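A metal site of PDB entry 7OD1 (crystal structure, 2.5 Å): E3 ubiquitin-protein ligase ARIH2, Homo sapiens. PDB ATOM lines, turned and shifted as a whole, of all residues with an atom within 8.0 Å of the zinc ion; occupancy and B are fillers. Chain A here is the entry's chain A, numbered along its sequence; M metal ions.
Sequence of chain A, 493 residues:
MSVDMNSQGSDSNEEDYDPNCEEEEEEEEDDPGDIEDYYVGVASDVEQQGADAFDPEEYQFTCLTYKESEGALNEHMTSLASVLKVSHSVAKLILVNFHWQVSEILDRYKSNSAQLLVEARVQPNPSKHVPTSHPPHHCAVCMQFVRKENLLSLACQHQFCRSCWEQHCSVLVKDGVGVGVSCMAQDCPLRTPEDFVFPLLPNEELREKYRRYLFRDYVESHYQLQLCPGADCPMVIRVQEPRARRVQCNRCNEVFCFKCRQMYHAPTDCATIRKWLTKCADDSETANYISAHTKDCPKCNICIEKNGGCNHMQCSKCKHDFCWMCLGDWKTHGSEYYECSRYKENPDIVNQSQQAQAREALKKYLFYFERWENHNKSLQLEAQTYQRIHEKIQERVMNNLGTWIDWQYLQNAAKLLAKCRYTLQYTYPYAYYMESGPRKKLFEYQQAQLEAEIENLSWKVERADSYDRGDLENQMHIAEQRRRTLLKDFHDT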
ATOM      1  N   PRO A 124     -35.760  19.129 -15.492  1.00  0.00           N
ATOM      2  CA  PRO A 124     -35.848  17.745 -15.979  1.00  0.00           C
ATOM      3  C   PRO A 124     -37.261  17.410 -16.444  1.00  0.00           C
ATOM      4  O   PRO A 124     -38.245  18.018 -16.020  1.00  0.00           O
ATOM      5  CB  PRO A 124     -35.443  16.910 -14.764  1.00  0.00           C
ATOM      6  CG  PRO A 124     -35.831  17.750 -13.599  1.00  0.00           C
ATOM      7  CD  PRO A 124     -35.644  19.184 -14.023  1.00  0.00           C
ATOM      8  N   SER A 153     -25.989  20.035  -6.894  1.00  0.00           N
ATOM      9  CA  SER A 153     -26.853  19.424  -7.893  1.00  0.00           C
ATOM     10  C   SER A 153     -27.571  20.524  -8.669  1.00  0.00           C
ATOM     11  O   SER A 153     -27.647  21.674  -8.229  1.00  0.00           O
ATOM     12  CB  SER A 153     -27.885  18.479  -7.259  1.00  0.00           C
ATOM     13  OG  SER A 153     -28.813  19.195  -6.463  1.00  0.00           O
ATOM     14  N   LEU A 154     -28.088  20.146  -9.841  1.00  0.00           N
ATOM     15  CA  LEU A 154     -28.933  21.016 -10.624  1.00  0.00           C
ATOM     16  C   LEU A 154     -30.392  20.704 -10.318  1.00  0.00           C
ATOM     17  O   LEU A 154     -30.712  19.985  -9.362  1.00  0.00           O
ATOM     18  CB  LEU A 154     -28.612  20.867 -12.121  1.00  0.00           C
ATOM     19  CG  LEU A 154     -27.129  20.934 -12.505  1.00  0.00           C
ATOM     20  CD1 LEU A 154     -26.942  20.642 -13.978  1.00  0.00           C
ATOM     21  CD2 LEU A 154     -26.537  22.292 -12.143  1.00  0.00           C
ATOM     22  N   ALA A 155     -31.311  21.236 -11.126  1.00  0.00           N
ATOM     23  CA  ALA A 155     -32.742  21.015 -10.896  1.00  0.00           C
ATOM     24  C   ALA A 155     -33.116  19.535 -10.987  1.00  0.00           C
ATOM     25  O   ALA A 155     -34.151  19.139 -10.436  1.00  0.00           O
ATOM     26  CB  ALA A 155     -33.571  21.825 -11.890  1.00  0.00           C
ATOM     27  N   CYS A 156     -32.304  18.730 -11.659  1.00  0.00           N
ATOM     28  CA  CYS A 156     -32.529  17.285 -11.736  1.00  0.00           C
ATOM     29  C   CYS A 156     -32.308  16.577 -10.418  1.00  0.00           C
ATOM     30  O   CYS A 156     -32.690  15.414 -10.286  1.00  0.00           O
ATOM     31  CB  CYS A 156     -31.615  16.677 -12.800  1.00  0.00           C
ATOM     32  SG  CYS A 156     -29.858  16.921 -12.432  1.00  0.00           S
ATOM     33  N   GLN A 157     -31.685  17.255  -9.445  1.00  0.00           N
ATOM     34  CA  GLN A 157     -31.387  16.740  -8.107  1.00  0.00           C
ATOM     35  C   GLN A 157     -30.356  15.616  -8.107  1.00  0.00           C
ATOM     36  O   GLN A 157     -30.205  14.930  -7.089  1.00  0.00           O
ATOM     37  CB  GLN A 157     -32.655  16.278  -7.374  1.00  0.00           C
ATOM     38  CG  GLN A 157     -33.704  17.368  -7.208  1.00  0.00           C
ATOM     39  CD  GLN A 157     -33.765  17.896  -5.790  1.00  0.00           C
ATOM     40  OE1 GLN A 157     -34.634  17.504  -5.009  1.00  0.00           O
ATOM     41  NE2 GLN A 157     -32.843  18.785  -5.443  1.00  0.00           N
ATOM     42  N   HIS A 158     -29.635  15.408  -9.211  1.00  0.00           N
ATOM     43  CA  HIS A 158     -28.501  14.490  -9.214  1.00  0.00           C
ATOM     44  C   HIS A 158     -27.359  15.117  -8.432  1.00  0.00           C
ATOM     45  O   HIS A 158     -26.690  16.040  -8.928  1.00  0.00           O
ATOM     46  CB  HIS A 158     -28.070  14.167 -10.640  1.00  0.00           C
ATOM     47  CG  HIS A 158     -29.132  13.498 -11.470  1.00  0.00           C
ATOM     48  ND1 HIS A 158     -29.201  13.639 -12.839  1.00  0.00           N
ATOM     49  CD2 HIS A 158     -30.152  12.682 -11.115  1.00  0.00           C
ATOM     50  CE1 HIS A 158     -30.217  12.932 -13.294  1.00  0.00           C
ATOM     51  NE2 HIS A 158     -30.816  12.355 -12.269  1.00  0.00           N
ATOM     52  N   GLN A 159     -27.114  14.615  -7.226  1.00  0.00           N
ATOM     53  CA  GLN A 159     -26.142  15.237  -6.330  1.00  0.00           C
ATOM     54  C   GLN A 159     -24.764  14.617  -6.486  1.00  0.00           C
ATOM     55  O   GLN A 159     -24.612  13.401  -6.584  1.00  0.00           O
ATOM     56  CB  GLN A 159     -26.614  15.118  -4.875  1.00  0.00           C
ATOM     57  CG  GLN A 159     -27.461  16.282  -4.413  1.00  0.00           C
ATOM     58  CD  GLN A 159     -28.572  15.864  -3.474  1.00  0.00           C
ATOM     59  OE1 GLN A 159     -28.389  15.772  -2.271  1.00  0.00           O
ATOM     60  NE2 GLN A 159     -29.755  15.592  -4.038  1.00  0.00           N
ATOM     61  N   PHE A 160     -23.743  15.491  -6.522  1.00  0.00           N
ATOM     62  CA  PHE A 160     -22.350  15.077  -6.562  1.00  0.00           C
ATOM     63  C   PHE A 160     -21.542  16.042  -5.704  1.00  0.00           C
ATOM     64  O   PHE A 160     -21.958  17.172  -5.445  1.00  0.00           O
ATOM     65  CB  PHE A 160     -21.806  15.054  -7.997  1.00  0.00           C
ATOM     66  CG  PHE A 160     -22.593  14.194  -8.941  1.00  0.00           C
ATOM     67  CD1 PHE A 160     -23.659  14.722  -9.650  1.00  0.00           C
ATOM     68  CD2 PHE A 160     -22.282  12.854  -9.104  1.00  0.00           C
ATOM     69  CE1 PHE A 160     -24.391  13.928 -10.525  1.00  0.00           C
ATOM     70  CE2 PHE A 160     -23.015  12.059  -9.969  1.00  0.00           C
ATOM     71  CZ  PHE A 160     -24.069  12.597 -10.684  1.00  0.00           C
ATOM     72  N   TRP A 165     -17.389  18.114  -8.987  1.00  0.00           N
ATOM     73  CA  TRP A 165     -17.933  19.155  -9.841  1.00  0.00           C
ATOM     74  C   TRP A 165     -16.830  20.068 -10.365  1.00  0.00           C
ATOM     75  O   TRP A 165     -16.819  20.428 -11.550  1.00  0.00           O
ATOM     76  CB  TRP A 165     -18.981  19.974  -9.083  1.00  0.00           C
ATOM     77  CG  TRP A 165     -20.385  19.448  -9.207  1.00  0.00           C
ATOM     78  CD1 TRP A 165     -21.152  18.936  -8.207  1.00  0.00           C
ATOM     79  CD2 TRP A 165     -21.181  19.414 -10.395  1.00  0.00           C
ATOM     80  NE1 TRP A 165     -22.382  18.571  -8.709  1.00  0.00           N
ATOM     81  CE2 TRP A 165     -22.426  18.857 -10.048  1.00  0.00           C
ATOM     82  CE3 TRP A 165     -20.971  19.794 -11.728  1.00  0.00           C
ATOM     83  CZ2 TRP A 165     -23.452  18.671 -10.971  1.00  0.00           C
ATOM     84  CZ3 TRP A 165     -21.986  19.616 -12.647  1.00  0.00           C
ATOM     85  CH2 TRP A 165     -23.216  19.057 -12.266  1.00  0.00           C
ATOM     86  N   SER A 182     -22.747  19.867 -18.833  1.00  0.00           N
ATOM     87  CA  SER A 182     -23.995  19.202 -18.472  1.00  0.00           C
ATOM     88  C   SER A 182     -23.831  18.477 -17.137  1.00  0.00           C
ATOM     89  O   SER A 182     -22.770  18.488 -16.513  1.00  0.00           O
ATOM     90  CB  SER A 182     -24.434  18.233 -19.567  1.00  0.00           C
ATOM     91  OG  SER A 182     -23.449  17.244 -19.793  1.00  0.00           O
ATOM     92  N   CYS A 183     -24.920  17.830 -16.711  1.00  0.00           N
ATOM     93  CA  CYS A 183     -24.919  17.046 -15.483  1.00  0.00           C
ATOM     94  C   CYS A 183     -23.988  15.843 -15.625  1.00  0.00           C
ATOM     95  O   CYS A 183     -23.825  15.276 -16.700  1.00  0.00           O
ATOM     96  CB  CYS A 183     -26.339  16.592 -15.142  1.00  0.00           C
ATOM     97  SG  CYS A 183     -26.520  15.755 -13.542  1.00  0.00           S
ATOM     98  N   MET A 184     -23.391  15.452 -14.495  1.00  0.00           N
ATOM     99  CA  MET A 184     -22.427  14.359 -14.489  1.00  0.00           C
ATOM    100  C   MET A 184     -23.071  12.981 -14.562  1.00  0.00           C
ATOM    101  O   MET A 184     -22.354  11.992 -14.710  1.00  0.00           O
ATOM    102  CB  MET A 184     -21.544  14.448 -13.250  1.00  0.00           C
ATOM    103  CG  MET A 184     -21.072  15.855 -12.918  1.00  0.00           C
ATOM    104  SD  MET A 184     -19.601  15.868 -11.895  1.00  0.00           S
ATOM    105  CE  MET A 184     -18.681  14.496 -12.594  1.00  0.00           C
ATOM    106  N   ALA A 185     -24.398  12.901 -14.446  1.00  0.00           N
ATOM    107  CA  ALA A 185     -25.099  11.626 -14.556  1.00  0.00           C
ATOM    108  C   ALA A 185     -25.379  11.314 -16.024  1.00  0.00           C
ATOM    109  O   ALA A 185     -25.757  12.212 -16.800  1.00  0.00           O
ATOM    110  CB  ALA A 185     -26.400  11.656 -13.758  1.00  0.00           C
ATOM    111  N   GLN A 186     -25.201  10.053 -16.390  1.00  0.00           N
ATOM    112  CA  GLN A 186     -25.488   9.618 -17.754  1.00  0.00           C
ATOM    113  C   GLN A 186     -26.930   9.924 -18.127  1.00  0.00           C
ATOM    114  O   GLN A 186     -27.825   9.916 -17.276  1.00  0.00           O
ATOM    115  CB  GLN A 186     -25.224   8.112 -17.894  1.00  0.00           C
ATOM    116  CG  GLN A 186     -25.041   7.620 -19.323  1.00  0.00           C
ATOM    117  CD  GLN A 186     -23.708   8.026 -19.933  1.00  0.00           C
ATOM    118  OE1 GLN A 186     -22.690   8.076 -19.234  1.00  0.00           O
ATOM    119  NE2 GLN A 186     -23.700   8.301 -21.223  1.00  0.00           N
ATOM    120  N   ASP A 187     -27.141  10.241 -19.405  1.00  0.00           N
ATOM    121  CA  ASP A 187     -28.452  10.434 -20.013  1.00  0.00           C
ATOM    122  C   ASP A 187     -29.069  11.780 -19.621  1.00  0.00           C
ATOM    123  O   ASP A 187     -29.854  12.341 -20.387  1.00  0.00           O
ATOM    124  CB  ASP A 187     -29.379   9.265 -19.656  1.00  0.00           C
ATOM    125  CG  ASP A 187     -30.753   9.358 -20.321  1.00  0.00           C
ATOM    126  OD1 ASP A 187     -31.529  10.267 -20.004  1.00  0.00           O
ATOM    127  OD2 ASP A 187     -31.038   8.490 -21.186  1.00  0.00           O
ATOM    128  N   CYS A 188     -28.726  12.313 -18.453  1.00  0.00           N
ATOM    129  CA  CYS A 188     -29.359  13.540 -17.968  1.00  0.00           C
ATOM    130  C   CYS A 188     -29.085  14.706 -18.914  1.00  0.00           C
ATOM    131  O   CYS A 188     -27.918  15.067 -19.115  1.00  0.00           O
ATOM    132  CB  CYS A 188     -28.868  13.880 -16.570  1.00  0.00           C
ATOM    133  SG  CYS A 188     -29.744  15.311 -15.879  1.00  0.00           S
ATOM    134  N   PRO A 189     -30.121  15.326 -19.481  1.00  0.00           N
ATOM    135  CA  PRO A 189     -29.892  16.402 -20.458  1.00  0.00           C
ATOM    136  C   PRO A 189     -29.659  17.772 -19.854  1.00  0.00           C
ATOM    137  O   PRO A 189     -29.364  18.710 -20.602  1.00  0.00           O
ATOM    138  CB  PRO A 189     -31.196  16.388 -21.273  1.00  0.00           C
ATOM    139  CG  PRO A 189     -32.231  15.966 -20.289  1.00  0.00           C
ATOM    140  CD  PRO A 189     -31.549  15.012 -19.336  1.00  0.00           C
ATOM    141  N   LEU A 190     -29.760  17.925 -18.536  1.00  0.00           N
ATOM    142  CA  LEU A 190     -29.668  19.255 -17.936  1.00  0.00           C
ATOM    143  C   LEU A 190     -28.286  19.859 -18.153  1.00  0.00           C
ATOM    144  O   LEU A 190     -27.267  19.168 -18.110  1.00  0.00           O
ATOM    145  CB  LEU A 190     -29.980  19.193 -16.439  1.00  0.00           C
ATOM    146  CG  LEU A 190     -31.450  19.381 -16.072  1.00  0.00           C
ATOM    147  CD1 LEU A 190     -32.231  18.098 -16.293  1.00  0.00           C
ATOM    148  CD2 LEU A 190     -31.584  19.864 -14.636  1.00  0.00           C
ATOM    149  N   ARG A 191     -28.272  21.166 -18.400  1.00  0.00           N
ATOM    150  CA  ARG A 191     -27.044  21.914 -18.629  1.00  0.00           C
ATOM    151  C   ARG A 191     -26.785  22.858 -17.457  1.00  0.00           C
ATOM    152  O   ARG A 191     -27.710  23.439 -16.893  1.00  0.00           O
ATOM    153  CB  ARG A 191     -27.125  22.720 -19.928  1.00  0.00           C
ATOM    154  CG  ARG A 191     -26.324  22.112 -21.076  1.00  0.00           C
ATOM    155  CD  ARG A 191     -26.355  23.006 -22.302  1.00  0.00           C
ATOM    156  NE  ARG A 191     -26.201  22.242 -23.533  1.00  0.00           N
ATOM    157  CZ  ARG A 191     -26.376  22.726 -24.752  1.00  0.00           C
ATOM    158  NH1 ARG A 191     -26.737  23.985 -24.952  1.00  0.00           N
ATOM    159  NH2 ARG A 191     -26.189  21.938 -25.804  1.00  0.00           N
HETATM  160 ZN    ZN M   1     -28.781  15.389 -13.781  1.00  0.00          ZN
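The zinc ion is bound by a ring nitrogen (ND1) of His 158 (2.0 Å), the side-chain sulfur (SG) of Cys 183 (2.3 Å), the side-chain sulfur (SG) of Cys 156 (2.3 Å) and the side-chain sulfur (SG) of Cys 188 (2.3 Å).
Four residues have an atom within 4 Å of the zinc ion: Cys 156, His 158, Cys 183 and Cys 188.
N of Cys 183 is in hydrogen-bond range of O of Leu 190, 3.0 Å away. N of Leu 190 sits close to SG of Cys 188 (3.7 Å). N of Ala 185 sits close to SG of Cys 183.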
